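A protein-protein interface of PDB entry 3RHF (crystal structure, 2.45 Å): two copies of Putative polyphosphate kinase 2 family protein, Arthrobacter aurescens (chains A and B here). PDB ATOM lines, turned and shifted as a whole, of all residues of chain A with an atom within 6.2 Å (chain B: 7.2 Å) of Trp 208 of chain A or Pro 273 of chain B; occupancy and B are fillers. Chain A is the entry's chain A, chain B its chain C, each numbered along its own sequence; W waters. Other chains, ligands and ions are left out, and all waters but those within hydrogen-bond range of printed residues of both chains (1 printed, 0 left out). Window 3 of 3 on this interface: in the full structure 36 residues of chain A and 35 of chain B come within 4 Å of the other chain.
Printed residues of chain B within 4 Å of Trp 208 of chain A: Glu 62, Ala 66, Lys 69, Phe 70, Trp 272 and Pro 273. Printed residues of chain B within 4 Å of Ser 205 of chain A: Trp 272 (3.4 Å). Printed residues of chain A within 4 Å of Glu 62 of chain B: Trp 208 and Lys 209. The nearest printed residue of chain B that does not touch Trp 208 of chain A is Phe 65 of chain B (4.1 Å). The nearest printed residue of chain A that does not touch Pro 273 of chain B is His 207 of chain A (4.4 Å).
ND1 of His 207 of chain A lies within hydrogen-bond range of NZ of Lys 274 of chain B (3.0 Å). OE2 of Glu 62 of chain B lies within salt-bridge range of NZ of Lys 209 of chain A, at 3.8 Å.
NE1 of Trp 208 of chain A sits at hydrogen-bond distance from O of Ser 205 of chain A, 3.2 Å away.
Trp 272 of chain B touches Ser 205 of chain A (NE1 to CB, 3.4 Å). His 207 of chain A touches Ala 275 of chain B. Glu 62 of chain B touches Trp 208 of chain A. CD2 of Trp 208 of chain A touches CB of Ala 66 of chain B, at 3.4 Å. Trp 208 of chain A touches Lys 69 of chain B. Trp 208 of chain A touches Phe 70 of chain B (O to CE2, 3.7 Å). Trp 208 of chain A touches Trp 272 of chain B. Trp 208 of chain A touches Pro 273 of chain B (CB to CG, 3.99 Å).
Water W1 lies within hydrogen-bond range of O of Pro 204 of chain A (2.5 Å), O of Pro 273 of chain B (2.9 Å), N of Trp 208 of chain A (2.9 Å) and N of His 207 of chain A (3.2 Å).
Of the 15 printed residues of chain B, 8 touch a printed residue of chain A. Hydrophobic or aromatic side chains of chain B within 4 Å of the printed part of chain A: Ala 66, Phe 70, Trp 272, Pro 273 and Ala 275. Of the 7 printed residues of chain A, 4 touch a printed residue of chain B. Hydrophobic or aromatic side chains of chain A within 4 Å of the printed part of chain B: His 207 and Trp 208. Along chain A the printed residues that touch a printed residue of chain B span positions 205 to 209. Among the printed residues, Asp or Glu carboxylates within 4 Å of a Lys or Arg side-chain nitrogen of the other chain: Lys 209 of chain A with Glu 62 of chain B (3.8 Å).
No position is printed for both chains. Of the 10 pairs that touch across the chains among the printed residues, none has its exchanged pair printed and touching as well.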
ATOM      1  N   PRO A 204      -9.413  -0.747 -14.325  1.00  0.00           N
ATOM      2  CA  PRO A 204      -9.404  -1.069 -15.769  1.00  0.00           C
ATOM      3  C   PRO A 204     -10.320  -2.217 -16.134  1.00  0.00           C
ATOM      4  O   PRO A 204     -10.931  -2.215 -17.195  1.00  0.00           O
ATOM      5  CB  PRO A 204      -7.947  -1.495 -16.054  1.00  0.00           C
ATOM      6  CG  PRO A 204      -7.142  -0.853 -14.999  1.00  0.00           C
ATOM      7  CD  PRO A 204      -8.045  -0.677 -13.771  1.00  0.00           C
ATOM      8  N   SER A 205     -10.383  -3.206 -15.269  1.00  0.00           N
ATOM      9  CA  SER A 205     -11.287  -4.311 -15.471  1.00  0.00           C
ATOM     10  C   SER A 205     -12.738  -3.839 -15.518  1.00  0.00           C
ATOM     11  O   SER A 205     -13.589  -4.570 -15.992  1.00  0.00           O
ATOM     12  CB  SER A 205     -11.103  -5.392 -14.385  1.00  0.00           C
ATOM     13  OG  SER A 205     -11.913  -5.131 -13.251  1.00  0.00           O
ATOM     14  N   LYS A 206     -13.019  -2.637 -15.030  1.00  0.00           N
ATOM     15  CA  LYS A 206     -14.409  -2.132 -14.998  1.00  0.00           C
ATOM     16  C   LYS A 206     -14.755  -0.989 -15.932  1.00  0.00           C
ATOM     17  O   LYS A 206     -15.891  -0.567 -15.951  1.00  0.00           O
ATOM     18  CB  LYS A 206     -14.809  -1.741 -13.570  1.00  0.00           C
ATOM     19  CG  LYS A 206     -14.840  -2.943 -12.666  1.00  0.00           C
ATOM     20  CD  LYS A 206     -15.312  -2.628 -11.255  1.00  0.00           C
ATOM     21  CE  LYS A 206     -15.372  -3.912 -10.387  1.00  0.00           C
ATOM     22  NZ  LYS A 206     -15.873  -3.532  -9.013  1.00  0.00           N
ATOM     23  N   HIS A 207     -13.802  -0.486 -16.711  1.00  0.00           N
ATOM     24  CA  HIS A 207     -14.103   0.556 -17.696  1.00  0.00           C
ATOM     25  C   HIS A 207     -15.238   0.187 -18.632  1.00  0.00           C
ATOM     26  O   HIS A 207     -16.087   1.009 -18.891  1.00  0.00           O
ATOM     27  CB  HIS A 207     -12.865   0.888 -18.495  1.00  0.00           C
ATOM     28  CG  HIS A 207     -11.839   1.622 -17.697  1.00  0.00           C
ATOM     29  ND1 HIS A 207     -10.500   1.620 -18.016  1.00  0.00           N
ATOM     30  CD2 HIS A 207     -11.957   2.365 -16.569  1.00  0.00           C
ATOM     31  CE1 HIS A 207      -9.835   2.321 -17.114  1.00  0.00           C
ATOM     32  NE2 HIS A 207     -10.695   2.791 -16.229  1.00  0.00           N
ATOM     33  N   TRP A 208     -15.281  -1.063 -19.114  1.00  0.00           N
ATOM     34  CA  TRP A 208     -16.363  -1.471 -20.026  1.00  0.00           C
ATOM     35  C   TRP A 208     -17.771  -1.209 -19.461  1.00  0.00           C
ATOM     36  O   TRP A 208     -18.715  -1.078 -20.236  1.00  0.00           O
ATOM     37  CB  TRP A 208     -16.237  -2.936 -20.425  1.00  0.00           C
ATOM     38  CG  TRP A 208     -16.532  -3.869 -19.340  1.00  0.00           C
ATOM     39  CD1 TRP A 208     -15.661  -4.329 -18.433  1.00  0.00           C
ATOM     40  CD2 TRP A 208     -17.785  -4.471 -19.040  1.00  0.00           C
ATOM     41  NE1 TRP A 208     -16.273  -5.181 -17.576  1.00  0.00           N
ATOM     42  CE2 TRP A 208     -17.588  -5.292 -17.928  1.00  0.00           C
ATOM     43  CE3 TRP A 208     -19.059  -4.382 -19.596  1.00  0.00           C
ATOM     44  CZ2 TRP A 208     -18.616  -6.030 -17.345  1.00  0.00           C
ATOM     45  CZ3 TRP A 208     -20.089  -5.118 -19.020  1.00  0.00           C
ATOM     46  CH2 TRP A 208     -19.862  -5.933 -17.908  1.00  0.00           C
ATOM     47  N   LYS A 209     -17.913  -1.134 -18.140  1.00  0.00           N
ATOM     48  CA  LYS A 209     -19.231  -0.932 -17.539  1.00  0.00           C
ATOM     49  C   LYS A 209     -19.589   0.518 -17.331  1.00  0.00           C
ATOM     50  O   LYS A 209     -20.725   0.804 -17.024  1.00  0.00           O
ATOM     51  CB  LYS A 209     -19.319  -1.545 -16.134  1.00  0.00           C
ATOM     52  CG  LYS A 209     -19.308  -3.003 -16.066  1.00  0.00           C
ATOM     53  CD  LYS A 209     -18.874  -3.518 -14.657  1.00  0.00           C
ATOM     54  CE  LYS A 209     -20.021  -4.214 -13.887  1.00  0.00           C
ATOM     55  NZ  LYS A 209     -19.473  -5.114 -12.837  1.00  0.00           N
ATOM     56  N   TYR A 210     -18.627   1.429 -17.385  1.00  0.00           N
ATOM     57  CA  TYR A 210     -18.934   2.805 -17.002  1.00  0.00           C
ATOM     58  C   TYR A 210     -19.872   3.427 -18.042  1.00  0.00           C
ATOM     59  O   TYR A 210     -19.675   3.264 -19.235  1.00  0.00           O
ATOM     60  CB  TYR A 210     -17.682   3.661 -16.816  1.00  0.00           C
ATOM     61  CG  TYR A 210     -18.043   5.103 -16.556  1.00  0.00           C
ATOM     62  CD1 TYR A 210     -18.262   5.564 -15.278  1.00  0.00           C
ATOM     63  CD2 TYR A 210     -18.242   5.979 -17.607  1.00  0.00           C
ATOM     64  CE1 TYR A 210     -18.651   6.855 -15.043  1.00  0.00           C
ATOM     65  CE2 TYR A 210     -18.613   7.260 -17.386  1.00  0.00           C
ATOM     66  CZ  TYR A 210     -18.817   7.716 -16.104  1.00  0.00           C
ATOM     67  OH  TYR A 210     -19.165   9.061 -15.914  1.00  0.00           O
ATOM     68  N   GLU B  62     -17.286 -13.008 -17.960  1.00  0.00           N
ATOM     69  CA  GLU B  62     -17.520 -11.549 -17.913  1.00  0.00           C
ATOM     70  C   GLU B  62     -16.689 -10.841 -18.989  1.00  0.00           C
ATOM     71  O   GLU B  62     -17.173  -9.944 -19.684  1.00  0.00           O
ATOM     72  CB  GLU B  62     -17.185 -11.012 -16.536  1.00  0.00           C
ATOM     73  CG  GLU B  62     -17.356  -9.497 -16.377  1.00  0.00           C
ATOM     74  CD  GLU B  62     -17.223  -9.012 -14.915  1.00  0.00           C
ATOM     75  OE1 GLU B  62     -16.615  -9.710 -14.076  1.00  0.00           O
ATOM     76  OE2 GLU B  62     -17.735  -7.933 -14.600  1.00  0.00           O
ATOM     77  N   LYS B  63     -15.452 -11.268 -19.165  1.00  0.00           N
ATOM     78  CA  LYS B  63     -14.629 -10.756 -20.277  1.00  0.00           C
ATOM     79  C   LYS B  63     -15.282 -11.056 -21.613  1.00  0.00           C
ATOM     80  O   LYS B  63     -15.336 -10.201 -22.484  1.00  0.00           O
ATOM     81  CB  LYS B  63     -13.186 -11.356 -20.282  1.00  0.00           C
ATOM     82  CG  LYS B  63     -12.235 -10.836 -19.193  1.00  0.00           C
ATOM     83  CD  LYS B  63     -10.776 -11.394 -19.371  1.00  0.00           C
ATOM     84  CE  LYS B  63      -9.827 -10.940 -18.275  1.00  0.00           C
ATOM     85  NZ  LYS B  63      -8.793 -11.943 -17.954  1.00  0.00           N
ATOM     86  N   PHE B  65     -18.336 -11.394 -22.359  1.00  0.00           N
ATOM     87  CA  PHE B  65     -19.460 -10.514 -22.440  1.00  0.00           C
ATOM     88  C   PHE B  65     -19.039  -9.077 -22.680  1.00  0.00           C
ATOM     89  O   PHE B  65     -19.556  -8.430 -23.586  1.00  0.00           O
ATOM     90  CB  PHE B  65     -20.221 -10.603 -21.134  1.00  0.00           C
ATOM     91  CG  PHE B  65     -21.516  -9.850 -21.126  1.00  0.00           C
ATOM     92  CD1 PHE B  65     -22.682 -10.457 -21.573  1.00  0.00           C
ATOM     93  CD2 PHE B  65     -21.565  -8.566 -20.665  1.00  0.00           C
ATOM     94  CE1 PHE B  65     -23.900  -9.793 -21.558  1.00  0.00           C
ATOM     95  CE2 PHE B  65     -22.761  -7.871 -20.635  1.00  0.00           C
ATOM     96  CZ  PHE B  65     -23.949  -8.474 -21.085  1.00  0.00           C
ATOM     97  N   ALA B  66     -18.109  -8.561 -21.882  1.00  0.00           N
ATOM     98  CA  ALA B  66     -17.584  -7.200 -22.146  1.00  0.00           C
ATOM     99  C   ALA B  66     -17.093  -7.092 -23.591  1.00  0.00           C
ATOM    100  O   ALA B  66     -17.379  -6.122 -24.263  1.00  0.00           O
ATOM    101  CB  ALA B  66     -16.458  -6.804 -21.155  1.00  0.00           C
ATOM    102  N   GLU B  67     -16.385  -8.091 -24.096  1.00  0.00           N
ATOM    103  CA  GLU B  67     -15.893  -7.974 -25.461  1.00  0.00           C
ATOM    104  C   GLU B  67     -17.043  -7.939 -26.429  1.00  0.00           C
ATOM    105  O   GLU B  67     -17.026  -7.215 -27.416  1.00  0.00           O
ATOM    106  CB  GLU B  67     -14.904  -9.067 -25.792  1.00  0.00           C
ATOM    107  CG  GLU B  67     -13.533  -8.850 -25.093  1.00  0.00           C
ATOM    108  CD  GLU B  67     -12.353  -9.066 -26.022  1.00  0.00           C
ATOM    109  OE1 GLU B  67     -12.505  -8.630 -27.174  1.00  0.00           O
ATOM    110  OE2 GLU B  67     -11.287  -9.629 -25.632  1.00  0.00           O
ATOM    111  N   GLY B  68     -18.086  -8.685 -26.100  1.00  0.00           N
ATOM    112  CA  GLY B  68     -19.236  -8.750 -26.968  1.00  0.00           C
ATOM    113  C   GLY B  68     -19.926  -7.410 -27.019  1.00  0.00           C
ATOM    114  O   GLY B  68     -20.305  -6.956 -28.096  1.00  0.00           O
ATOM    115  N   LYS B  69     -20.104  -6.803 -25.841  1.00  0.00           N
ATOM    116  CA  LYS B  69     -20.744  -5.497 -25.715  1.00  0.00           C
ATOM    117  C   LYS B  69     -20.026  -4.466 -26.594  1.00  0.00           C
ATOM    118  O   LYS B  69     -20.639  -3.565 -27.104  1.00  0.00           O
ATOM    119  CB  LYS B  69     -20.799  -5.040 -24.223  1.00  0.00           C
ATOM    120  CG  LYS B  69     -21.215  -3.564 -23.997  1.00  0.00           C
ATOM    121  CD  LYS B  69     -21.444  -3.132 -22.494  1.00  0.00           C
ATOM    122  CE  LYS B  69     -22.200  -1.743 -22.398  1.00  0.00           C
ATOM    123  NZ  LYS B  69     -22.328  -1.149 -20.993  1.00  0.00           N
ATOM    124  N   PHE B  70     -18.731  -4.650 -26.792  1.00  0.00           N
ATOM    125  CA  PHE B  70     -17.914  -3.736 -27.594  1.00  0.00           C
ATOM    126  C   PHE B  70     -17.648  -4.228 -29.013  1.00  0.00           C
ATOM    127  O   PHE B  70     -16.738  -3.742 -29.661  1.00  0.00           O
ATOM    128  CB  PHE B  70     -16.581  -3.478 -26.862  1.00  0.00           C
ATOM    129  CG  PHE B  70     -16.663  -2.389 -25.804  1.00  0.00           C
ATOM    130  CD1 PHE B  70     -15.937  -1.191 -25.957  1.00  0.00           C
ATOM    131  CD2 PHE B  70     -17.444  -2.547 -24.690  1.00  0.00           C
ATOM    132  CE1 PHE B  70     -16.005  -0.180 -24.999  1.00  0.00           C
ATOM    133  CE2 PHE B  70     -17.537  -1.543 -23.754  1.00  0.00           C
ATOM    134  CZ  PHE B  70     -16.811  -0.352 -23.908  1.00  0.00           C
ATOM    135  N   ASP B 271      -9.681 -10.148 -23.369  1.00  0.00           N
ATOM    136  CA  ASP B 271      -9.355  -9.164 -22.359  1.00  0.00           C
ATOM    137  C   ASP B 271     -10.470  -8.202 -22.099  1.00  0.00           C
ATOM    138  O   ASP B 271     -11.376  -8.127 -22.829  1.00  0.00           O
ATOM    139  CB  ASP B 271      -8.156  -8.354 -22.751  1.00  0.00           C
ATOM    140  CG  ASP B 271      -7.138  -8.277 -21.667  1.00  0.00           C
ATOM    141  OD1 ASP B 271      -7.454  -8.352 -20.482  1.00  0.00           O
ATOM    142  OD2 ASP B 271      -5.984  -8.146 -22.008  1.00  0.00           O
ATOM    143  N   TRP B 272     -10.365  -7.442 -21.035  1.00  0.00           N
ATOM    144  CA  TRP B 272     -11.254  -6.331 -20.757  1.00  0.00           C
ATOM    145  C   TRP B 272     -11.095  -5.260 -21.824  1.00  0.00           C
ATOM    146  O   TRP B 272      -9.975  -4.929 -22.179  1.00  0.00           O
ATOM    147  CB  TRP B 272     -10.885  -5.698 -19.450  1.00  0.00           C
ATOM    148  CG  TRP B 272     -10.854  -6.611 -18.318  1.00  0.00           C
ATOM    149  CD1 TRP B 272      -9.772  -6.950 -17.587  1.00  0.00           C
ATOM    150  CD2 TRP B 272     -11.967  -7.284 -17.751  1.00  0.00           C
ATOM    151  NE1 TRP B 272     -10.132  -7.808 -16.584  1.00  0.00           N
ATOM    152  CE2 TRP B 272     -11.482  -8.028 -16.653  1.00  0.00           C
ATOM    153  CE3 TRP B 272     -13.327  -7.334 -18.058  1.00  0.00           C
ATOM    154  CZ2 TRP B 272     -12.317  -8.815 -15.844  1.00  0.00           C
ATOM    155  CZ3 TRP B 272     -14.148  -8.125 -17.283  1.00  0.00           C
ATOM    156  CH2 TRP B 272     -13.648  -8.856 -16.179  1.00  0.00           C
ATOM    157  N   PRO B 273     -12.204  -4.744 -22.364  1.00  0.00           N
ATOM    158  CA  PRO B 273     -12.145  -3.669 -23.309  1.00  0.00           C
ATOM    159  C   PRO B 273     -11.543  -2.406 -22.745  1.00  0.00           C
ATOM    160  O   PRO B 273     -11.720  -2.077 -21.574  1.00  0.00           O
ATOM    161  CB  PRO B 273     -13.608  -3.402 -23.617  1.00  0.00           C
ATOM    162  CG  PRO B 273     -14.220  -4.643 -23.421  1.00  0.00           C
ATOM    163  CD  PRO B 273     -13.564  -5.266 -22.278  1.00  0.00           C
ATOM    164  N   LYS B 274     -10.875  -1.688 -23.626  1.00  0.00           N
ATOM    165  CA  LYS B 274     -10.266  -0.436 -23.269  1.00  0.00           C
ATOM    166  C   LYS B 274     -11.318   0.644 -23.439  1.00  0.00           C
ATOM    167  O   LYS B 274     -12.128   0.594 -24.359  1.00  0.00           O
ATOM    168  CB  LYS B 274      -9.020  -0.191 -24.141  1.00  0.00           C
ATOM    169  CG  LYS B 274      -7.890   0.633 -23.463  1.00  0.00           C
ATOM    170  CD  LYS B 274      -7.540   0.288 -21.908  1.00  0.00           C
ATOM    171  CE  LYS B 274      -7.414   1.597 -20.993  1.00  0.00           C
ATOM    172  NZ  LYS B 274      -8.050   1.372 -19.664  1.00  0.00           N
ATOM    173  N   ALA B 275     -11.331   1.595 -22.507  1.00  0.00           N
ATOM    174  CA  ALA B 275     -12.243   2.748 -22.573  1.00  0.00           C
ATOM    175  C   ALA B 275     -11.889   3.596 -23.778  1.00  0.00           C
ATOM    176  O   ALA B 275     -10.715   3.925 -23.988  1.00  0.00           O
ATOM    177  CB  ALA B 275     -12.126   3.589 -21.312  1.00  0.00           C
ATOM    178  N   ASP B 276     -12.903   3.949 -24.566  1.00  0.00           N
ATOM    179  CA  ASP B 276     -12.723   4.842 -25.729  1.00  0.00           C
ATOM    180  C   ASP B 276     -13.095   6.281 -25.345  1.00  0.00           C
ATOM    181  O   ASP B 276     -13.966   6.872 -25.969  1.00  0.00           O
ATOM    182  CB  ASP B 276     -13.569   4.365 -26.932  1.00  0.00           C
ATOM    183  CG  ASP B 276     -15.003   4.025 -26.539  1.00  0.00           C
ATOM    184  OD1 ASP B 276     -15.615   3.103 -27.150  1.00  0.00           O
ATOM    185  OD2 ASP B 276     -15.498   4.662 -25.577  1.00  0.00           O
ATOM    186  N   PHE B 277     -12.444   6.807 -24.301  1.00  0.00           N
ATOM    187  CA  PHE B 277     -12.685   8.156 -23.778  1.00  0.00           C
ATOM    188  C   PHE B 277     -11.678   8.493 -22.675  1.00  0.00           C
ATOM    189  O   PHE B 277     -11.052   7.613 -22.086  1.00  0.00           O
ATOM    190  CB  PHE B 277     -14.116   8.312 -23.227  1.00  0.00           C
ATOM    191  CG  PHE B 277     -14.402   7.443 -22.040  1.00  0.00           C
ATOM    192  CD1 PHE B 277     -13.931   7.789 -20.782  1.00  0.00           C
ATOM    193  CD2 PHE B 277     -15.113   6.263 -22.181  1.00  0.00           C
ATOM    194  CE1 PHE B 277     -14.170   6.982 -19.696  1.00  0.00           C
ATOM    195  CE2 PHE B 277     -15.361   5.442 -21.087  1.00  0.00           C
ATOM    196  CZ  PHE B 277     -14.893   5.799 -19.850  1.00  0.00           C
HETATM  197  O   HOH W   1     -12.761  -2.582 -18.923  1.00  0.00           O
